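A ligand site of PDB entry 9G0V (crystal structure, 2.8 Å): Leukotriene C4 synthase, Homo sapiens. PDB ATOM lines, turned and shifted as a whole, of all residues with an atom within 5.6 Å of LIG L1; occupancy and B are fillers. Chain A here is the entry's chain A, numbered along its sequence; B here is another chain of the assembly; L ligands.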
ATOM      1  N   ARG A  58       2.999  20.034  -7.626  1.00  0.00           N
ATOM      2  CA  ARG A  58       1.826  20.752  -7.120  1.00  0.00           C
ATOM      3  C   ARG A  58       1.902  21.024  -5.624  1.00  0.00           C
ATOM      4  O   ARG A  58       1.384  22.036  -5.158  1.00  0.00           O
ATOM      5  CB  ARG A  58       0.533  19.992  -7.458  1.00  0.00           C
ATOM      6  CG  ARG A  58      -0.700  20.868  -7.444  1.00  0.00           C
ATOM      7  CD  ARG A  58      -1.250  21.092  -8.839  1.00  0.00           C
ATOM      8  NE  ARG A  58      -0.369  21.867  -9.718  1.00  0.00           N
ATOM      9  CZ  ARG A  58      -0.259  23.197  -9.691  1.00  0.00           C
ATOM     10  NH1 ARG A  58      -0.965  23.909  -8.817  1.00  0.00           N
ATOM     11  NH2 ARG A  58       0.545  23.818 -10.536  1.00  0.00           N
ATOM     12  N   ASN A  62       1.646  25.017  -4.062  1.00  0.00           N
ATOM     13  CA  ASN A  62       0.745  25.327  -2.956  1.00  0.00           C
ATOM     14  C   ASN A  62       1.487  25.892  -1.763  1.00  0.00           C
ATOM     15  O   ASN A  62       1.065  26.903  -1.201  1.00  0.00           O
ATOM     16  CB  ASN A  62      -0.042  24.089  -2.545  1.00  0.00           C
ATOM     17  CG  ASN A  62      -1.315  23.950  -3.319  1.00  0.00           C
ATOM     18  OD1 ASN A  62      -2.329  24.570  -2.959  1.00  0.00           O
ATOM     19  ND2 ASN A  62      -1.287  23.186  -4.403  1.00  0.00           N
ATOM     20  N   GLU A  65       2.575  29.504  -2.388  1.00  0.00           N
ATOM     21  CA  GLU A  65       1.420  30.384  -2.359  1.00  0.00           C
ATOM     22  C   GLU A  65       1.026  30.724  -0.920  1.00  0.00           C
ATOM     23  O   GLU A  65       0.651  31.850  -0.610  1.00  0.00           O
ATOM     24  CB  GLU A  65       0.303  29.657  -3.088  1.00  0.00           C
ATOM     25  CG  GLU A  65      -1.094  30.207  -2.906  1.00  0.00           C
ATOM     26  CD  GLU A  65      -2.048  29.316  -3.655  1.00  0.00           C
ATOM     27  OE1 GLU A  65      -2.921  28.704  -2.991  1.00  0.00           O
ATOM     28  OE2 GLU A  65      -1.913  29.202  -4.892  1.00  0.00           O
ATOM     29  N   TYR A  66       1.135  29.746  -0.035  1.00  0.00           N
ATOM     30  CA  TYR A  66       0.817  29.916   1.358  1.00  0.00           C
ATOM     31  C   TYR A  66       1.903  30.583   2.177  1.00  0.00           C
ATOM     32  O   TYR A  66       1.617  31.111   3.255  1.00  0.00           O
ATOM     33  CB  TYR A  66       0.422  28.571   1.946  1.00  0.00           C
ATOM     34  CG  TYR A  66      -1.042  28.318   1.740  1.00  0.00           C
ATOM     35  CD1 TYR A  66      -1.536  27.949   0.511  1.00  0.00           C
ATOM     36  CD2 TYR A  66      -1.954  28.622   2.741  1.00  0.00           C
ATOM     37  CE1 TYR A  66      -2.895  27.798   0.296  1.00  0.00           C
ATOM     38  CE2 TYR A  66      -3.318  28.476   2.537  1.00  0.00           C
ATOM     39  CZ  TYR A  66      -3.782  28.077   1.307  1.00  0.00           C
ATOM     40  OH  TYR A  66      -5.140  27.939   1.127  1.00  0.00           O
ATOM     41  N   TYR A 100       2.785  17.616   4.646  1.00  0.00           N
ATOM     42  CA  TYR A 100       1.908  17.793   3.494  1.00  0.00           C
ATOM     43  C   TYR A 100       2.707  17.463   2.233  1.00  0.00           C
ATOM     44  O   TYR A 100       2.206  16.748   1.363  1.00  0.00           O
ATOM     45  CB  TYR A 100       1.389  19.252   3.432  1.00  0.00           C
ATOM     46  CG  TYR A 100       0.767  19.674   2.112  1.00  0.00           C
ATOM     47  CD1 TYR A 100       1.556  20.223   1.101  1.00  0.00           C
ATOM     48  CD2 TYR A 100      -0.601  19.599   1.909  1.00  0.00           C
ATOM     49  CE1 TYR A 100       0.997  20.598  -0.113  1.00  0.00           C
ATOM     50  CE2 TYR A 100      -1.170  20.009   0.717  1.00  0.00           C
ATOM     51  CZ  TYR A 100      -0.368  20.496  -0.303  1.00  0.00           C
ATOM     52  OH  TYR A 100      -0.922  20.900  -1.488  1.00  0.00           O
ATOM     53  N   TYR A 104       1.933  14.343  -0.190  1.00  0.00           N
ATOM     54  CA  TYR A 104       1.656  14.556  -1.611  1.00  0.00           C
ATOM     55  C   TYR A 104       2.672  13.786  -2.485  1.00  0.00           C
ATOM     56  O   TYR A 104       2.341  13.375  -3.593  1.00  0.00           O
ATOM     57  CB  TYR A 104       1.676  16.057  -1.923  1.00  0.00           C
ATOM     58  CG  TYR A 104       0.562  16.554  -2.826  1.00  0.00           C
ATOM     59  CD1 TYR A 104      -0.028  15.718  -3.745  1.00  0.00           C
ATOM     60  CD2 TYR A 104       0.150  17.870  -2.781  1.00  0.00           C
ATOM     61  CE1 TYR A 104      -1.029  16.172  -4.607  1.00  0.00           C
ATOM     62  CE2 TYR A 104      -0.839  18.341  -3.639  1.00  0.00           C
ATOM     63  CZ  TYR A 104      -1.431  17.487  -4.542  1.00  0.00           C
ATOM     64  OH  TYR A 104      -2.422  17.958  -5.369  1.00  0.00           O
ATOM     65  N   ARG A 111      -1.908  13.565   1.546  1.00  0.00           N
ATOM     66  CA  ARG A 111      -1.649  14.980   1.827  1.00  0.00           C
ATOM     67  C   ARG A 111      -2.815  15.669   2.574  1.00  0.00           C
ATOM     68  O   ARG A 111      -2.625  16.710   3.189  1.00  0.00           O
ATOM     69  CB  ARG A 111      -1.246  15.744   0.544  1.00  0.00           C
ATOM     70  CG  ARG A 111      -2.266  16.720  -0.037  1.00  0.00           C
ATOM     71  CD  ARG A 111      -2.807  16.287  -1.374  1.00  0.00           C
ATOM     72  NE  ARG A 111      -3.749  17.246  -1.946  1.00  0.00           N
ATOM     73  CZ  ARG A 111      -5.050  17.269  -1.687  1.00  0.00           C
ATOM     74  NH1 ARG A 111      -5.832  18.169  -2.268  1.00  0.00           N
ATOM     75  NH2 ARG A 111      -5.589  16.386  -0.857  1.00  0.00           N
ATOM     76  N   LEU A 115      -2.665  18.778   5.506  1.00  0.00           N
ATOM     77  CA  LEU A 115      -3.181  20.023   4.942  1.00  0.00           C
ATOM     78  C   LEU A 115      -4.138  20.650   5.947  1.00  0.00           C
ATOM     79  O   LEU A 115      -4.103  21.861   6.154  1.00  0.00           O
ATOM     80  CB  LEU A 115      -3.873  19.799   3.583  1.00  0.00           C
ATOM     81  CG  LEU A 115      -4.623  21.004   3.048  1.00  0.00           C
ATOM     82  CD1 LEU A 115      -3.671  22.038   2.459  1.00  0.00           C
ATOM     83  CD2 LEU A 115      -5.743  20.615   2.136  1.00  0.00           C
ATOM     84  N   PHE B  29     -10.834  33.286  -1.414  1.00  0.00           N
ATOM     85  CA  PHE B  29     -10.490  32.836  -2.757  1.00  0.00           C
ATOM     86  C   PHE B  29     -10.110  31.356  -2.805  1.00  0.00           C
ATOM     87  O   PHE B  29     -10.292  30.731  -3.842  1.00  0.00           O
ATOM     88  CB  PHE B  29      -9.356  33.691  -3.361  1.00  0.00           C
ATOM     89  CG  PHE B  29      -9.651  35.146  -3.588  1.00  0.00           C
ATOM     90  CD1 PHE B  29     -10.951  35.623  -3.519  1.00  0.00           C
ATOM     91  CD2 PHE B  29      -8.649  36.029  -3.901  1.00  0.00           C
ATOM     92  CE1 PHE B  29     -11.224  36.972  -3.717  1.00  0.00           C
ATOM     93  CE2 PHE B  29      -8.919  37.376  -4.121  1.00  0.00           C
ATOM     94  CZ  PHE B  29     -10.203  37.841  -4.025  1.00  0.00           C
ATOM     95  N   SER B  30      -9.600  30.796  -1.704  1.00  0.00           N
ATOM     96  CA  SER B  30      -9.281  29.366  -1.649  1.00  0.00           C
ATOM     97  C   SER B  30     -10.578  28.555  -1.458  1.00  0.00           C
ATOM     98  O   SER B  30     -10.729  27.461  -2.029  1.00  0.00           O
ATOM     99  CB  SER B  30      -8.294  29.083  -0.527  1.00  0.00           C
ATOM    100  OG  SER B  30      -6.985  29.509  -0.885  1.00  0.00           O
ATOM    101  N   LEU B  31     -11.509  29.084  -0.651  1.00  0.00           N
ATOM    102  CA  LEU B  31     -12.818  28.490  -0.406  1.00  0.00           C
ATOM    103  C   LEU B  31     -13.598  28.417  -1.723  1.00  0.00           C
ATOM    104  O   LEU B  31     -14.290  27.435  -1.966  1.00  0.00           O
ATOM    105  CB  LEU B  31     -13.583  29.345   0.619  1.00  0.00           C
ATOM    106  CG  LEU B  31     -14.851  28.729   1.211  1.00  0.00           C
ATOM    107  CD1 LEU B  31     -14.521  27.579   2.131  1.00  0.00           C
ATOM    108  CD2 LEU B  31     -15.656  29.779   1.952  1.00  0.00           C
ATOM    109  N   VAL B  33     -12.216  28.407  -4.923  1.00  0.00           N
ATOM    110  CA  VAL B  33     -11.573  27.466  -5.838  1.00  0.00           C
ATOM    111  C   VAL B  33     -11.841  26.019  -5.406  1.00  0.00           C
ATOM    112  O   VAL B  33     -12.057  25.164  -6.257  1.00  0.00           O
ATOM    113  CB  VAL B  33     -10.082  27.794  -6.052  1.00  0.00           C
ATOM    114  CG1 VAL B  33      -9.305  26.628  -6.646  1.00  0.00           C
ATOM    115  CG2 VAL B  33      -9.930  29.023  -6.936  1.00  0.00           C
ATOM    116  N   ILE B  34     -11.908  25.757  -4.087  1.00  0.00           N
ATOM    117  CA  ILE B  34     -12.207  24.419  -3.599  1.00  0.00           C
ATOM    118  C   ILE B  34     -13.688  24.045  -3.870  1.00  0.00           C
ATOM    119  O   ILE B  34     -13.986  22.859  -4.007  1.00  0.00           O
ATOM    120  CB  ILE B  34     -11.767  24.234  -2.121  1.00  0.00           C
ATOM    121  CG1 ILE B  34     -11.014  22.893  -1.929  1.00  0.00           C
ATOM    122  CG2 ILE B  34     -12.916  24.386  -1.125  1.00  0.00           C
ATOM    123  CD1 ILE B  34      -9.805  22.689  -2.882  1.00  0.00           C
ATOM    124  N   ARG B  37     -13.787  22.841  -7.604  1.00  0.00           N
ATOM    125  CA  ARG B  37     -13.225  21.500  -7.742  1.00  0.00           C
ATOM    126  C   ARG B  37     -14.292  20.430  -7.457  1.00  0.00           C
ATOM    127  O   ARG B  37     -14.287  19.371  -8.073  1.00  0.00           O
ATOM    128  CB  ARG B  37     -12.020  21.327  -6.814  1.00  0.00           C
ATOM    129  CG  ARG B  37     -10.834  22.165  -7.239  1.00  0.00           C
ATOM    130  CD  ARG B  37      -9.564  21.767  -6.529  1.00  0.00           C
ATOM    131  NE  ARG B  37      -8.398  22.258  -7.254  1.00  0.00           N
ATOM    132  CZ  ARG B  37      -7.728  21.575  -8.168  1.00  0.00           C
ATOM    133  NH1 ARG B  37      -6.689  22.112  -8.785  1.00  0.00           N
ATOM    134  NH2 ARG B  37      -8.095  20.331  -8.463  1.00  0.00           N
ATOM    135  N   PRO B  44      -7.364  17.118  -7.764  1.00  0.00           N
ATOM    136  CA  PRO B  44      -5.939  17.494  -7.665  1.00  0.00           C
ATOM    137  C   PRO B  44      -5.020  16.300  -7.966  1.00  0.00           C
ATOM    138  O   PRO B  44      -5.403  15.176  -7.648  1.00  0.00           O
ATOM    139  CB  PRO B  44      -5.782  17.937  -6.209  1.00  0.00           C
ATOM    140  CG  PRO B  44      -7.177  18.018  -5.642  1.00  0.00           C
ATOM    141  CD  PRO B  44      -7.993  17.053  -6.435  1.00  0.00           C
ATOM    142  N   PRO B  45      -3.840  16.484  -8.583  1.00  0.00           N
ATOM    143  CA  PRO B  45      -3.183  17.745  -8.966  1.00  0.00           C
ATOM    144  C   PRO B  45      -3.551  18.334 -10.331  1.00  0.00           C
ATOM    145  O   PRO B  45      -2.675  18.920 -10.983  1.00  0.00           O
ATOM    146  CB  PRO B  45      -1.704  17.361  -8.928  1.00  0.00           C
ATOM    147  CG  PRO B  45      -1.699  15.961  -9.434  1.00  0.00           C
ATOM    148  CD  PRO B  45      -2.940  15.336  -8.838  1.00  0.00           C
ATOM    149  N   LEU B  46      -4.794  18.196 -10.772  1.00  0.00           N
ATOM    150  CA  LEU B  46      -5.203  18.747 -12.061  1.00  0.00           C
ATOM    151  C   LEU B  46      -5.638  20.191 -11.935  1.00  0.00           C
ATOM    152  O   LEU B  46      -6.476  20.512 -11.103  1.00  0.00           O
ATOM    153  CB  LEU B  46      -6.308  17.927 -12.714  1.00  0.00           C
ATOM    154  CG  LEU B  46      -5.851  16.799 -13.585  1.00  0.00           C
ATOM    155  CD1 LEU B  46      -7.003  15.890 -13.916  1.00  0.00           C
ATOM    156  CD2 LEU B  46      -5.197  17.320 -14.855  1.00  0.00           C
ATOM    157  N   THR B  47      -5.076  21.055 -12.773  1.00  0.00           N
ATOM    158  CA  THR B  47      -5.431  22.480 -12.773  1.00  0.00           C
ATOM    159  C   THR B  47      -6.306  22.867 -14.000  1.00  0.00           C
ATOM    160  O   THR B  47      -6.708  24.026 -14.117  1.00  0.00           O
ATOM    161  CB  THR B  47      -4.160  23.335 -12.678  1.00  0.00           C
ATOM    162  OG1 THR B  47      -3.474  23.345 -13.923  1.00  0.00           O
ATOM    163  CG2 THR B  47      -3.225  22.877 -11.561  1.00  0.00           C
ATOM    164  N   TYR B  57     -10.018  29.292 -10.948  1.00  0.00           N
ATOM    165  CA  TYR B  57      -8.699  28.829 -10.533  1.00  0.00           C
ATOM    166  C   TYR B  57      -7.615  29.856 -10.874  1.00  0.00           C
ATOM    167  O   TYR B  57      -6.738  30.119 -10.052  1.00  0.00           O
ATOM    168  CB  TYR B  57      -8.382  27.469 -11.179  1.00  0.00           C
ATOM    169  CG  TYR B  57      -6.969  27.006 -10.919  1.00  0.00           C
ATOM    170  CD1 TYR B  57      -6.574  26.569  -9.668  1.00  0.00           C
ATOM    171  CD2 TYR B  57      -6.005  27.061 -11.922  1.00  0.00           C
ATOM    172  CE1 TYR B  57      -5.258  26.218  -9.408  1.00  0.00           C
ATOM    173  CE2 TYR B  57      -4.691  26.716 -11.681  1.00  0.00           C
ATOM    174  CZ  TYR B  57      -4.327  26.270 -10.420  1.00  0.00           C
ATOM    175  OH  TYR B  57      -3.020  25.917 -10.171  1.00  0.00           O
ATOM    176  N   GLN B  60      -7.517  33.067  -8.682  1.00  0.00           N
ATOM    177  CA  GLN B  60      -6.895  32.813  -7.396  1.00  0.00           C
ATOM    178  C   GLN B  60      -5.365  32.811  -7.500  1.00  0.00           C
ATOM    179  O   GLN B  60      -4.704  33.365  -6.628  1.00  0.00           O
ATOM    180  CB  GLN B  60      -7.419  31.477  -6.847  1.00  0.00           C
ATOM    181  CG  GLN B  60      -6.809  31.034  -5.522  1.00  0.00           C
ATOM    182  CD  GLN B  60      -5.668  30.084  -5.727  1.00  0.00           C
ATOM    183  OE1 GLN B  60      -4.539  30.349  -5.323  1.00  0.00           O
ATOM    184  NE2 GLN B  60      -5.931  28.959  -6.403  1.00  0.00           N
HETATM  185  N1  LIG L   1      -4.894  26.946  -4.006  1.00  0.00           N
HETATM  186  C1  LIG L   1      -5.924  26.278  -3.167  1.00  0.00           C
HETATM  187  C2  LIG L   1      -7.305  26.823  -3.542  1.00  0.00           C
HETATM  188  O1  LIG L   1      -7.365  27.977  -4.003  1.00  0.00           O
HETATM  189  O2  LIG L   1      -8.292  26.056  -3.363  1.00  0.00           O
HETATM  190  C3  LIG L   1      -5.639  26.511  -1.689  1.00  0.00           C
HETATM  191  C4  LIG L   1      -6.381  25.562  -0.737  1.00  0.00           C
HETATM  192  C5  LIG L   1      -6.173  24.099  -1.059  1.00  0.00           C
HETATM  193  O3  LIG L   1      -7.085  23.293  -0.960  1.00  0.00           O
HETATM  194  N2  LIG L   1      -4.926  23.758  -1.408  1.00  0.00           N
HETATM  195  C6  LIG L   1      -4.525  22.480  -1.973  1.00  0.00           C
HETATM  196  C7  LIG L   1      -5.263  22.146  -3.266  1.00  0.00           C
HETATM  197  O4  LIG L   1      -6.309  21.508  -3.253  1.00  0.00           O
HETATM  198  C8  LIG L   1      -4.681  21.340  -0.968  1.00  0.00           C
HETATM  199  S1  LIG L   1      -3.534  19.984  -1.252  1.00  0.00           S
HETATM  200  N3  LIG L   1      -4.689  22.580  -4.387  1.00  0.00           N
HETATM  201  C9  LIG L   1      -5.183  22.223  -5.686  1.00  0.00           C
HETATM  202  C10 LIG L   1      -4.278  21.213  -6.371  1.00  0.00           C
HETATM  203  O5  LIG L   1      -4.341  21.100  -7.602  1.00  0.00           O
HETATM  204  O6  LIG L   1      -3.517  20.548  -5.625  1.00  0.00           O
HETATM  205  C1  LG2 L   2      -9.540  28.360   2.959  1.00  0.00           C
HETATM  206  C2  LG2 L   2     -10.227  26.264   4.102  1.00  0.00           C
HETATM  207  C3  LG2 L   2      -7.152  25.357   2.664  1.00  0.00           C
HETATM  208  C4  LG2 L   2      -6.498  28.468   4.802  1.00  0.00           C
HETATM  209  C5  LG2 L   2      -6.125  29.507   3.938  1.00  0.00           C
HETATM  210  C6  LG2 L   2      -5.985  30.828   4.357  1.00  0.00           C
HETATM  211  C7  LG2 L   2      -6.244  31.130   5.680  1.00  0.00           C
HETATM  212  C8  LG2 L   2      -6.609  30.114   6.561  1.00  0.00           C
HETATM  213  C9  LG2 L   2      -6.730  28.778   6.146  1.00  0.00           C
HETATM  214  C10 LG2 L   2     -11.514  28.315   4.413  1.00  0.00           C
HETATM  215  C11 LG2 L   2     -11.849  29.627   4.106  1.00  0.00           C
HETATM  216  C12 LG2 L   2     -12.911  30.245   4.782  1.00  0.00           C
HETATM  217  C13 LG2 L   2     -13.229  28.294   6.032  1.00  0.00           C
HETATM  218  C14 LG2 L   2     -13.435  32.414   5.610  1.00  0.00           C
HETATM  219  C15 LG2 L   2     -13.076  33.843   5.175  1.00  0.00           C
HETATM  220  N1  LG2 L   2     -10.476  27.666   3.824  1.00  0.00           N
HETATM  221  C16 LG2 L   2      -8.752  25.957   4.508  1.00  0.00           C
HETATM  222  C17 LG2 L   2      -7.666  26.544   3.547  1.00  0.00           C
HETATM  223  C18 LG2 L   2      -8.360  27.462   2.494  1.00  0.00           C
HETATM  224  N2  LG2 L   2      -6.514  27.122   4.313  1.00  0.00           N
HETATM  225  C19 LG2 L   2      -5.369  26.409   4.522  1.00  0.00           C
HETATM  226  C20 LG2 L   2      -5.144  24.975   4.071  1.00  0.00           C
HETATM  227  C21 LG2 L   2      -6.373  24.287   3.457  1.00  0.00           C
HETATM  228  O1  LG2 L   2      -4.422  26.881   5.138  1.00  0.00           O
HETATM  229  F1  LG2 L   2      -6.828  30.436   7.824  1.00  0.00           F
HETATM  230  F2  LG2 L   2      -6.157  32.379   6.113  1.00  0.00           F
HETATM  231  N3  LG2 L   2     -13.577  29.549   5.729  1.00  0.00           N
HETATM  232  N4  LG2 L   2     -12.206  27.700   5.397  1.00  0.00           N
HETATM  233  O2  LG2 L   2     -13.255  31.552   4.473  1.00  0.00           O
HETATM  234  F3  LG2 L   2     -11.761  34.068   5.416  1.00  0.00           F
HETATM  235  F4  LG2 L   2     -13.312  33.992   3.837  1.00  0.00           F
HETATM  236  F5  LG2 L   2     -13.839  34.720   5.893  1.00  0.00           F
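O5 of LIG L1 is in salt-bridge range of NH1 of Arg 37 of chain B (2.8 Å). OG of Ser 30 of chain B sits close to O1 of LIG L1, at 3.5 Å. The side-chain hydroxyl (OH) of Tyr 100 lies close to a sulfur (S1) of LIG L1. NE of Arg 111 sits close to S1 of LIG L1 (2.8 Å). An oxygen (O1) of LIG L1 lies within hydrogen-bond range of the side-chain amide nitrogen of Gln 60 of chain B, at 3.0 Å. A nitrogen (N2) of LIG L1 is in hydrogen-bond range of the side-chain amide oxygen (OD1) of Asn 62, 3.1 Å away. The side-chain carboxylate (OE1) of Glu 65 is in salt-bridge range of a nitrogen (N1) of LIG L1 (2.8 Å). The side-chain hydroxyl (OH) of Tyr 104 sits at hydrogen-bond distance from an oxygen (O6) of LIG L1 (2.8 Å).
The side-chain carboxylate of Glu 65 lies close to the side-chain amide oxygen of Gln 60 of chain B, 2.9 Å away. The guanidinium group (NH1) of Arg 58 is in hydrogen-bond range of the side-chain hydroxyl (OH) of Tyr 57 of chain B, 3.2 Å away. The backbone carbonyl oxygen (O) of Leu 46 of chain B sits at hydrogen-bond distance from the guanidinium group (NH1) of Arg 37 of chain B, at 2.8 Å. The side-chain amide nitrogen of Asn 62 sits at hydrogen-bond distance from the backbone carbonyl oxygen of Arg 58 (3.0 Å). The side-chain hydroxyl (OH) of Tyr 66 sits at hydrogen-bond distance from the side-chain hydroxyl (OG) of Ser 30 of chain B (3.1 Å).
CD of Arg 58 touches O5 of LIG L1, 3.3 Å away. OH of Tyr 66 touches C3 of LIG L1, at 3.2 Å. Leu 115 touches LIG L1. Val 33 of chain B touches LIG L1. CD1 of Ile 34 of chain B touches O3 of LIG L1 (3.4 Å). Pro 44 of chain B touches LIG L1 (CB to O6, 3.5 Å). CA of Pro 45 of chain B touches O5 of LIG L1, at 3.8 Å. Hydrophobic or aromatic side chains that line LIG L1: Tyr 66, Tyr 100, Tyr 104, Leu 115, Val 33 of chain B, Ile 34 of chain B and Pro 44 of chain B. Within 4 Å of LIG L1: Arg 58, Asn 62, Glu 65, Tyr 66, Tyr 100, Tyr 104, Arg 111, Leu 115, Ser 30 of chain B, Val 33 of chain B, Ile 34 of chain B, Arg 37 of chain B, Pro 44 of chain B, Pro 45 of chain B and Gln 60 of chain B. The nearest printed residue that does not touch LIG L1 is Phe 29 of chain B (4.02 Å).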
